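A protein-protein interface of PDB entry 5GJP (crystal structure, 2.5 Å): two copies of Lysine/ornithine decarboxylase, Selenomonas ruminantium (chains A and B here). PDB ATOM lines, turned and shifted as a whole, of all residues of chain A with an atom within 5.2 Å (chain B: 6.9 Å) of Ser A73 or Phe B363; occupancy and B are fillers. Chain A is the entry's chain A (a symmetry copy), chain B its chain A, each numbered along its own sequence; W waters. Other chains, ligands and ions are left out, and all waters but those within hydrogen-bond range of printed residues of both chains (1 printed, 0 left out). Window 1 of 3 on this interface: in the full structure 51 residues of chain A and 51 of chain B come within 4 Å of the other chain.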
ATOM      1  N   VAL A  71     -14.996   8.482  10.030  1.00  0.00           N
ATOM      2  CA  VAL A  71     -15.277   8.537   8.615  1.00  0.00           C
ATOM      3  C   VAL A  71     -15.768   9.922   8.269  1.00  0.00           C
ATOM      4  O   VAL A  71     -16.458  10.541   9.040  1.00  0.00           O
ATOM      5  CB  VAL A  71     -16.299   7.476   8.183  1.00  0.00           C
ATOM      6  CG1 VAL A  71     -15.880   6.108   8.669  1.00  0.00           C
ATOM      7  CG2 VAL A  71     -17.680   7.817   8.686  1.00  0.00           C
ATOM      8  N   ALA A  72     -15.356  10.422   7.122  1.00  0.00           N
ATOM      9  CA  ALA A  72     -15.717  11.780   6.709  1.00  0.00           C
ATOM     10  C   ALA A  72     -16.597  11.898   5.457  1.00  0.00           C
ATOM     11  O   ALA A  72     -16.906  13.001   5.086  1.00  0.00           O
ATOM     12  CB  ALA A  72     -14.464  12.604   6.508  1.00  0.00           C
ATOM     13  N   SER A  73     -16.978  10.787   4.827  1.00  0.00           N
ATOM     14  CA  SER A  73     -17.837  10.778   3.624  1.00  0.00           C
ATOM     15  C   SER A  73     -18.526   9.407   3.424  1.00  0.00           C
ATOM     16  O   SER A  73     -18.234   8.452   4.135  1.00  0.00           O
ATOM     17  CB  SER A  73     -17.012  11.095   2.370  1.00  0.00           C
ATOM     18  OG  SER A  73     -16.045  10.077   2.152  1.00  0.00           O
ATOM     19  N   ALA A  74     -19.418   9.331   2.447  1.00  0.00           N
ATOM     20  CA  ALA A  74     -20.016   8.060   2.025  1.00  0.00           C
ATOM     21  C   ALA A  74     -18.951   7.034   1.586  1.00  0.00           C
ATOM     22  O   ALA A  74     -19.033   5.852   1.949  1.00  0.00           O
ATOM     23  CB  ALA A  74     -21.058   8.269   0.917  1.00  0.00           C
ATOM     24  N   GLY A  75     -17.955   7.487   0.838  1.00  0.00           N
ATOM     25  CA  GLY A  75     -16.942   6.590   0.319  1.00  0.00           C
ATOM     26  C   GLY A  75     -16.108   5.939   1.410  1.00  0.00           C
ATOM     27  O   GLY A  75     -15.703   4.795   1.258  1.00  0.00           O
ATOM     28  N   GLU A  76     -15.867   6.660   2.508  1.00  0.00           N
ATOM     29  CA  GLU A  76     -15.079   6.114   3.614  1.00  0.00           C
ATOM     30  C   GLU A  76     -15.879   5.059   4.355  1.00  0.00           C
ATOM     31  O   GLU A  76     -15.347   3.992   4.676  1.00  0.00           O
ATOM     32  CB  GLU A  76     -14.532   7.215   4.542  1.00  0.00           C
ATOM     33  CG  GLU A  76     -13.308   7.940   3.949  1.00  0.00           C
ATOM     34  CD  GLU A  76     -12.608   8.928   4.900  1.00  0.00           C
ATOM     35  OE1 GLU A  76     -13.177   9.234   5.982  1.00  0.00           O
ATOM     36  OE2 GLU A  76     -11.474   9.406   4.566  1.00  0.00           O
ATOM     37  N   MET A  77     -17.161   5.343   4.578  1.00  0.00           N
ATOM     38  CA  MET A  77     -18.132   4.371   5.122  1.00  0.00           C
ATOM     39  C   MET A  77     -18.290   3.095   4.258  1.00  0.00           C
ATOM     40  O   MET A  77     -18.380   2.002   4.770  1.00  0.00           O
ATOM     41  CB  MET A  77     -19.503   5.037   5.285  1.00  0.00           C
ATOM     42  CG  MET A  77     -19.630   5.978   6.463  1.00  0.00           C
ATOM     43  SD  MET A  77     -21.278   6.748   6.523  1.00  0.00           S
ATOM     44  CE  MET A  77     -20.884   8.470   6.801  1.00  0.00           C
ATOM     45  N   TYR A  92     -19.201   9.569  12.158  1.00  0.00           N
ATOM     46  CA  TYR A  92     -19.283  10.467  11.021  1.00  0.00           C
ATOM     47  C   TYR A  92     -18.881  11.848  11.536  1.00  0.00           C
ATOM     48  O   TYR A  92     -19.718  12.609  12.005  1.00  0.00           O
ATOM     49  CB  TYR A  92     -20.675  10.444  10.403  1.00  0.00           C
ATOM     50  CG  TYR A  92     -20.825  11.115   9.052  1.00  0.00           C
ATOM     51  CD1 TYR A  92     -19.739  11.449   8.260  1.00  0.00           C
ATOM     52  CD2 TYR A  92     -22.087  11.367   8.530  1.00  0.00           C
ATOM     53  CE1 TYR A  92     -19.909  12.032   7.024  1.00  0.00           C
ATOM     54  CE2 TYR A  92     -22.258  11.946   7.283  1.00  0.00           C
ATOM     55  CZ  TYR A  92     -21.169  12.281   6.532  1.00  0.00           C
ATOM     56  OH  TYR A  92     -21.328  12.882   5.272  1.00  0.00           O
ATOM     57  N   ASN A  94     -17.007  14.448  10.005  1.00  0.00           N
ATOM     58  CA  ASN A  94     -17.110  15.627   9.183  1.00  0.00           C
ATOM     59  C   ASN A  94     -18.244  16.534   9.725  1.00  0.00           C
ATOM     60  O   ASN A  94     -19.413  16.132   9.686  1.00  0.00           O
ATOM     61  CB  ASN A  94     -17.424  15.247   7.721  1.00  0.00           C
ATOM     62  CG  ASN A  94     -17.154  16.370   6.783  1.00  0.00           C
ATOM     63  OD1 ASN A  94     -17.438  17.514   7.101  1.00  0.00           O
ATOM     64  ND2 ASN A  94     -16.547  16.069   5.632  1.00  0.00           N
ATOM     65  N   ASP A  98     -22.927  15.823   3.481  1.00  0.00           N
ATOM     66  CA  ASP A  98     -23.717  15.803   2.242  1.00  0.00           C
ATOM     67  C   ASP A  98     -24.862  14.797   2.318  1.00  0.00           C
ATOM     68  O   ASP A  98     -24.994  14.061   3.286  1.00  0.00           O
ATOM     69  CB  ASP A  98     -22.813  15.572   0.990  1.00  0.00           C
ATOM     70  CG  ASP A  98     -22.028  14.206   0.995  1.00  0.00           C
ATOM     71  OD1 ASP A  98     -22.240  13.343   1.884  1.00  0.00           O
ATOM     72  OD2 ASP A  98     -21.168  13.996   0.092  1.00  0.00           O
ATOM     73  N   GLY A 101     -23.758  11.122   2.219  1.00  0.00           N
ATOM     74  CA  GLY A 101     -23.166  10.727   3.480  1.00  0.00           C
ATOM     75  C   GLY A 101     -24.194  10.488   4.555  1.00  0.00           C
ATOM     76  O   GLY A 101     -24.088   9.524   5.289  1.00  0.00           O
ATOM     77  N   ILE B 272     -24.067  22.821   0.910  1.00  0.00           N
ATOM     78  CA  ILE B 272     -24.402  21.786   1.892  1.00  0.00           C
ATOM     79  C   ILE B 272     -24.313  22.220   3.335  1.00  0.00           C
ATOM     80  O   ILE B 272     -24.733  21.462   4.192  1.00  0.00           O
ATOM     81  CB  ILE B 272     -23.551  20.533   1.713  1.00  0.00           C
ATOM     82  CG1 ILE B 272     -22.063  20.815   1.952  1.00  0.00           C
ATOM     83  CG2 ILE B 272     -23.757  19.981   0.319  1.00  0.00           C
ATOM     84  CD1 ILE B 272     -21.199  19.568   1.862  1.00  0.00           C
ATOM     85  N   ASP B 286     -20.252  21.253  -1.997  1.00  0.00           N
ATOM     86  CA  ASP B 286     -19.922  19.837  -2.140  1.00  0.00           C
ATOM     87  C   ASP B 286     -18.793  19.485  -3.118  1.00  0.00           C
ATOM     88  O   ASP B 286     -18.478  18.329  -3.296  1.00  0.00           O
ATOM     89  CB  ASP B 286     -21.167  18.958  -2.356  1.00  0.00           C
ATOM     90  CG  ASP B 286     -21.939  19.295  -3.605  1.00  0.00           C
ATOM     91  OD1 ASP B 286     -21.458  20.051  -4.456  1.00  0.00           O
ATOM     92  OD2 ASP B 286     -23.058  18.787  -3.735  1.00  0.00           O
ATOM     93  N   GLU B 287     -18.198  20.487  -3.749  1.00  0.00           N
ATOM     94  CA  GLU B 287     -16.956  20.301  -4.481  1.00  0.00           C
ATOM     95  C   GLU B 287     -15.906  21.278  -3.970  1.00  0.00           C
ATOM     96  O   GLU B 287     -16.203  22.403  -3.663  1.00  0.00           O
ATOM     97  CB  GLU B 287     -17.146  20.410  -5.990  1.00  0.00           C
ATOM     98  CG  GLU B 287     -15.886  20.125  -6.792  1.00  0.00           C
ATOM     99  CD  GLU B 287     -15.647  18.648  -7.052  1.00  0.00           C
ATOM    100  OE1 GLU B 287     -16.208  17.811  -6.340  1.00  0.00           O
ATOM    101  OE2 GLU B 287     -14.884  18.313  -7.967  1.00  0.00           O
ATOM    102  N   TYR B 290      -9.789  19.700  -3.173  1.00  0.00           N
ATOM    103  CA  TYR B 290      -9.236  18.396  -3.425  1.00  0.00           C
ATOM    104  C   TYR B 290      -9.901  17.759  -4.627  1.00  0.00           C
ATOM    105  O   TYR B 290      -9.527  16.694  -5.045  1.00  0.00           O
ATOM    106  CB  TYR B 290      -9.370  17.517  -2.202  1.00  0.00           C
ATOM    107  CG  TYR B 290      -8.371  17.802  -1.123  1.00  0.00           C
ATOM    108  CD1 TYR B 290      -7.071  17.370  -1.229  1.00  0.00           C
ATOM    109  CD2 TYR B 290      -8.738  18.487   0.019  1.00  0.00           C
ATOM    110  CE1 TYR B 290      -6.164  17.617  -0.229  1.00  0.00           C
ATOM    111  CE2 TYR B 290      -7.838  18.737   1.020  1.00  0.00           C
ATOM    112  CZ  TYR B 290      -6.554  18.302   0.889  1.00  0.00           C
ATOM    113  OH  TYR B 290      -5.658  18.559   1.888  1.00  0.00           O
ATOM    114  N   GLY B 320     -14.929  24.035   0.871  1.00  0.00           N
ATOM    115  CA  GLY B 320     -15.193  22.742   0.276  1.00  0.00           C
ATOM    116  C   GLY B 320     -15.679  21.783   1.324  1.00  0.00           C
ATOM    117  O   GLY B 320     -15.709  22.109   2.497  1.00  0.00           O
ATOM    118  N   PRO B 321     -16.024  20.565   0.906  1.00  0.00           N
ATOM    119  CA  PRO B 321     -16.636  19.619   1.823  1.00  0.00           C
ATOM    120  C   PRO B 321     -15.647  18.894   2.745  1.00  0.00           C
ATOM    121  O   PRO B 321     -16.085  18.174   3.633  1.00  0.00           O
ATOM    122  CB  PRO B 321     -17.285  18.609   0.858  1.00  0.00           C
ATOM    123  CG  PRO B 321     -16.296  18.562  -0.265  1.00  0.00           C
ATOM    124  CD  PRO B 321     -15.681  19.933  -0.375  1.00  0.00           C
ATOM    125  N   SER B 322     -14.345  19.043   2.530  1.00  0.00           N
ATOM    126  CA  SER B 322     -13.377  18.282   3.329  1.00  0.00           C
ATOM    127  C   SER B 322     -13.103  18.847   4.728  1.00  0.00           C
ATOM    128  O   SER B 322     -13.460  19.991   5.046  1.00  0.00           O
ATOM    129  CB  SER B 322     -12.050  18.184   2.604  1.00  0.00           C
ATOM    130  OG  SER B 322     -11.270  19.287   2.945  1.00  0.00           O
ATOM    131  N   CYS B 323     -12.382  18.034   5.501  1.00  0.00           N
ATOM    132  CA  CYS B 323     -12.030  18.273   6.906  1.00  0.00           C
ATOM    133  C   CYS B 323     -10.714  19.014   7.076  1.00  0.00           C
ATOM    134  O   CYS B 323     -10.240  19.222   8.170  1.00  0.00           O
ATOM    135  CB  CYS B 323     -11.907  16.932   7.613  1.00  0.00           C
ATOM    136  SG  CYS B 323     -13.469  16.021   7.657  1.00  0.00           S
ATOM    137  N   ASP B 327      -9.120  23.837   2.675  1.00  0.00           N
ATOM    138  CA  ASP B 327     -10.221  23.714   1.702  1.00  0.00           C
ATOM    139  C   ASP B 327     -11.130  24.945   1.736  1.00  0.00           C
ATOM    140  O   ASP B 327     -12.300  24.861   2.098  1.00  0.00           O
ATOM    141  CB  ASP B 327     -11.020  22.418   1.962  1.00  0.00           C
ATOM    142  CG  ASP B 327     -11.817  21.922   0.713  1.00  0.00           C
ATOM    143  OD1 ASP B 327     -12.004  22.696  -0.269  1.00  0.00           O
ATOM    144  OD2 ASP B 327     -12.260  20.732   0.712  1.00  0.00           O
ATOM    145  N   THR B 358      -9.089  14.417  -6.711  1.00  0.00           N
ATOM    146  CA  THR B 358      -8.678  13.288  -5.899  1.00  0.00           C
ATOM    147  C   THR B 358      -9.890  12.693  -5.194  1.00  0.00           C
ATOM    148  O   THR B 358     -10.992  13.235  -5.272  1.00  0.00           O
ATOM    149  CB  THR B 358      -7.678  13.736  -4.815  1.00  0.00           C
ATOM    150  OG1 THR B 358      -8.366  14.517  -3.846  1.00  0.00           O
ATOM    151  CG2 THR B 358      -6.534  14.588  -5.372  1.00  0.00           C
ATOM    152  N   ARG B 359      -9.668  11.594  -4.481  1.00  0.00           N
ATOM    153  CA  ARG B 359     -10.674  10.987  -3.597  1.00  0.00           C
ATOM    154  C   ARG B 359     -10.311  11.193  -2.141  1.00  0.00           C
ATOM    155  O   ARG B 359     -10.686  10.398  -1.257  1.00  0.00           O
ATOM    156  CB  ARG B 359     -10.902   9.479  -3.924  1.00  0.00           C
ATOM    157  CG  ARG B 359     -11.468   9.275  -5.337  1.00  0.00           C
ATOM    158  CD  ARG B 359     -12.234   8.010  -5.508  1.00  0.00           C
ATOM    159  NE  ARG B 359     -13.227   7.887  -4.456  1.00  0.00           N
ATOM    160  CZ  ARG B 359     -13.709   6.731  -3.976  1.00  0.00           C
ATOM    161  NH1 ARG B 359     -13.337   5.563  -4.488  1.00  0.00           N
ATOM    162  NH2 ARG B 359     -14.570   6.736  -2.969  1.00  0.00           N
ATOM    163  N   PHE B 360      -9.606  12.295  -1.881  1.00  0.00           N
ATOM    164  CA  PHE B 360      -9.334  12.705  -0.510  1.00  0.00           C
ATOM    165  C   PHE B 360     -10.630  12.711   0.308  1.00  0.00           C
ATOM    166  O   PHE B 360     -11.682  13.110  -0.196  1.00  0.00           O
ATOM    167  CB  PHE B 360      -8.675  14.085  -0.489  1.00  0.00           C
ATOM    168  CG  PHE B 360      -8.060  14.415   0.823  1.00  0.00           C
ATOM    169  CD1 PHE B 360      -6.944  13.711   1.260  1.00  0.00           C
ATOM    170  CD2 PHE B 360      -8.603  15.385   1.638  1.00  0.00           C
ATOM    171  CE1 PHE B 360      -6.377  14.004   2.488  1.00  0.00           C
ATOM    172  CE2 PHE B 360      -8.045  15.686   2.852  1.00  0.00           C
ATOM    173  CZ  PHE B 360      -6.931  14.990   3.293  1.00  0.00           C
ATOM    174  N   ASN B 361     -10.546  12.271   1.557  1.00  0.00           N
ATOM    175  CA  ASN B 361     -11.719  12.105   2.462  1.00  0.00           C
ATOM    176  C   ASN B 361     -12.739  11.062   1.963  1.00  0.00           C
ATOM    177  O   ASN B 361     -13.875  11.055   2.403  1.00  0.00           O
ATOM    178  CB  ASN B 361     -12.434  13.457   2.755  1.00  0.00           C
ATOM    179  CG  ASN B 361     -11.747  14.279   3.817  1.00  0.00           C
ATOM    180  OD1 ASN B 361     -10.540  14.278   3.936  1.00  0.00           O
ATOM    181  ND2 ASN B 361     -12.522  14.983   4.598  1.00  0.00           N
ATOM    182  N   GLY B 362     -12.332  10.204   1.043  1.00  0.00           N
ATOM    183  CA  GLY B 362     -13.249   9.292   0.332  1.00  0.00           C
ATOM    184  C   GLY B 362     -14.299   9.865  -0.603  1.00  0.00           C
ATOM    185  O   GLY B 362     -15.189   9.115  -1.056  1.00  0.00           O
ATOM    186  N   PHE B 363     -14.240  11.165  -0.920  1.00  0.00           N
ATOM    187  CA  PHE B 363     -15.214  11.725  -1.854  1.00  0.00           C
ATOM    188  C   PHE B 363     -15.052  11.054  -3.220  1.00  0.00           C
ATOM    189  O   PHE B 363     -13.948  10.616  -3.559  1.00  0.00           O
ATOM    190  CB  PHE B 363     -15.112  13.250  -1.957  1.00  0.00           C
ATOM    191  CG  PHE B 363     -15.567  13.936  -0.716  1.00  0.00           C
ATOM    192  CD1 PHE B 363     -16.920  13.907  -0.353  1.00  0.00           C
ATOM    193  CD2 PHE B 363     -14.648  14.549   0.148  1.00  0.00           C
ATOM    194  CE1 PHE B 363     -17.344  14.503   0.822  1.00  0.00           C
ATOM    195  CE2 PHE B 363     -15.070  15.131   1.336  1.00  0.00           C
ATOM    196  CZ  PHE B 363     -16.415  15.112   1.667  1.00  0.00           C
ATOM    197  N   TYR B 364     -16.153  10.936  -3.972  1.00  0.00           N
ATOM    198  CA  TYR B 364     -16.095  10.418  -5.349  1.00  0.00           C
ATOM    199  C   TYR B 364     -15.663  11.533  -6.302  1.00  0.00           C
ATOM    200  O   TYR B 364     -15.965  12.693  -6.092  1.00  0.00           O
ATOM    201  CB  TYR B 364     -17.462   9.863  -5.795  1.00  0.00           C
ATOM    202  CG  TYR B 364     -18.064   8.835  -4.871  1.00  0.00           C
ATOM    203  CD1 TYR B 364     -17.415   7.627  -4.618  1.00  0.00           C
ATOM    204  CD2 TYR B 364     -19.282   9.076  -4.235  1.00  0.00           C
ATOM    205  CE1 TYR B 364     -17.961   6.681  -3.750  1.00  0.00           C
ATOM    206  CE2 TYR B 364     -19.843   8.141  -3.365  1.00  0.00           C
ATOM    207  CZ  TYR B 364     -19.189   6.942  -3.124  1.00  0.00           C
ATOM    208  OH  TYR B 364     -19.766   6.018  -2.270  1.00  0.00           O
ATOM    209  N   LEU B 365     -14.973  11.180  -7.364  1.00  0.00           N
ATOM    210  CA  LEU B 365     -14.671  12.135  -8.426  1.00  0.00           C
ATOM    211  C   LEU B 365     -16.003  12.665  -8.999  1.00  0.00           C
ATOM    212  O   LEU B 365     -16.936  11.916  -9.199  1.00  0.00           O
ATOM    213  CB  LEU B 365     -13.796  11.466  -9.506  1.00  0.00           C
ATOM    214  CG  LEU B 365     -12.406  10.954  -9.051  1.00  0.00           C
ATOM    215  CD1 LEU B 365     -11.680  10.096 -10.109  1.00  0.00           C
ATOM    216  CD2 LEU B 365     -11.479  12.099  -8.603  1.00  0.00           C
ATOM    217  N   ALA B 366     -16.134  13.963  -9.212  1.00  0.00           N
ATOM    218  CA  ALA B 366     -17.328  14.466  -9.866  1.00  0.00           C
ATOM    219  C   ALA B 366     -17.350  13.928 -11.304  1.00  0.00           C
ATOM    220  O   ALA B 366     -16.336  14.015 -12.006  1.00  0.00           O
ATOM    221  CB  ALA B 366     -17.315  15.969  -9.877  1.00  0.00           C
HETATM  222  O   HOH W   1     -18.100   9.669  -0.712  1.00  0.00           O
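The backbone carbonyl oxygen of Pro B321 is in hydrogen-bond range of the side-chain amide nitrogen of Asn A94, 2.9 Å away.
The side-chain sulfur of Cys B323 is in hydrogen-bond range of the side-chain amide nitrogen of Asn A94 (3.7 Å).
The backbone carbonyl oxygen (O) of Gly B362 sits close to the side-chain hydroxyl (OG) of Ser A73 (3.5 Å).
OG of Ser A73 sits close to O of Asn B361, 2.4 Å away.
The backbone carbonyl oxygen (O) of Gly B362 is in hydrogen-bond range of the guanidinium group (NH2) of Arg B359 (3.1 Å).
NE of Arg B359 sits at hydrogen-bond distance from O of Phe B363.
The backbone carbonyl oxygen (O) of Ala A72 sits at hydrogen-bond distance from the side-chain amide nitrogen (ND2) of Asn A94, at 3.1 Å.
The side-chain hydroxyl (OG) of Ser A73 lies close to the backbone NH (N) of Gly A75 (3.5 Å).
The side-chain hydroxyl of Ser A73 sits at hydrogen-bond distance from the backbone NH of Glu A76 (3.4 Å).
OD1 of Asp A98 is in hydrogen-bond range of N of Gly A101 (2.7 Å).
CB of Ala A72 touches SG of Cys B323, 3.7 Å away.
Ala A72 touches Asn B361.
Ser A73 touches Phe B363 (OG to N, 3.7 Å).
Gly B362 touches Gly A75.
Tyr B364 touches Gly A75.
Glu A76 touches Asn B361.
Gly B362 touches Glu A76 (N to OE2, 3.7 Å).
Asp A98 touches Phe B363 (OD2 to CE1, 3.9 Å).
Val A71 touches none of the printed residues of chain B.
Of the printed residues of chain B, Ala A72 touches Cys B323 (3.7 Å) and Asn B361 (3.6 Å).
Ser A73 touches just these residues of chain B: Asn B361 (2.4 Å), Gly B362 (3.3 Å) and Phe B363 (3.7 Å).
Ala A74 touches none of the printed residues of chain B.
Of the printed residues of chain B, Asp A98 touches Phe B363.
Printed residues of chain A within 4 Å of Asn B361: Ala A72 (3.6 Å), Ser A73 (2.4 Å) and Glu A76 (3.3 Å).
Of chain A, only Ser A73 and Asp A98 come within 4 Å of Phe B363.
Of the 11 printed residues of chain A, 6 touch a printed residue of chain B.
Hydrophobic or aromatic side chains of chain A within 4 Å of the printed part of chain B: Ala A72.
Among the printed residues, no Asp or Glu carboxylate lies within 4 Å of a Lys or Arg side-chain nitrogen of the other chain.
No position is printed for both chains.
Of the 12 pairs that touch across the chains among the printed residues, none has its exchanged pair printed and touching as well.
Water W1 lies within hydrogen-bond range of the backbone NH (N) of Gly A75, the backbone carbonyl oxygen (O) of Gly B362 and the backbone NH (N) of Ala A74.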
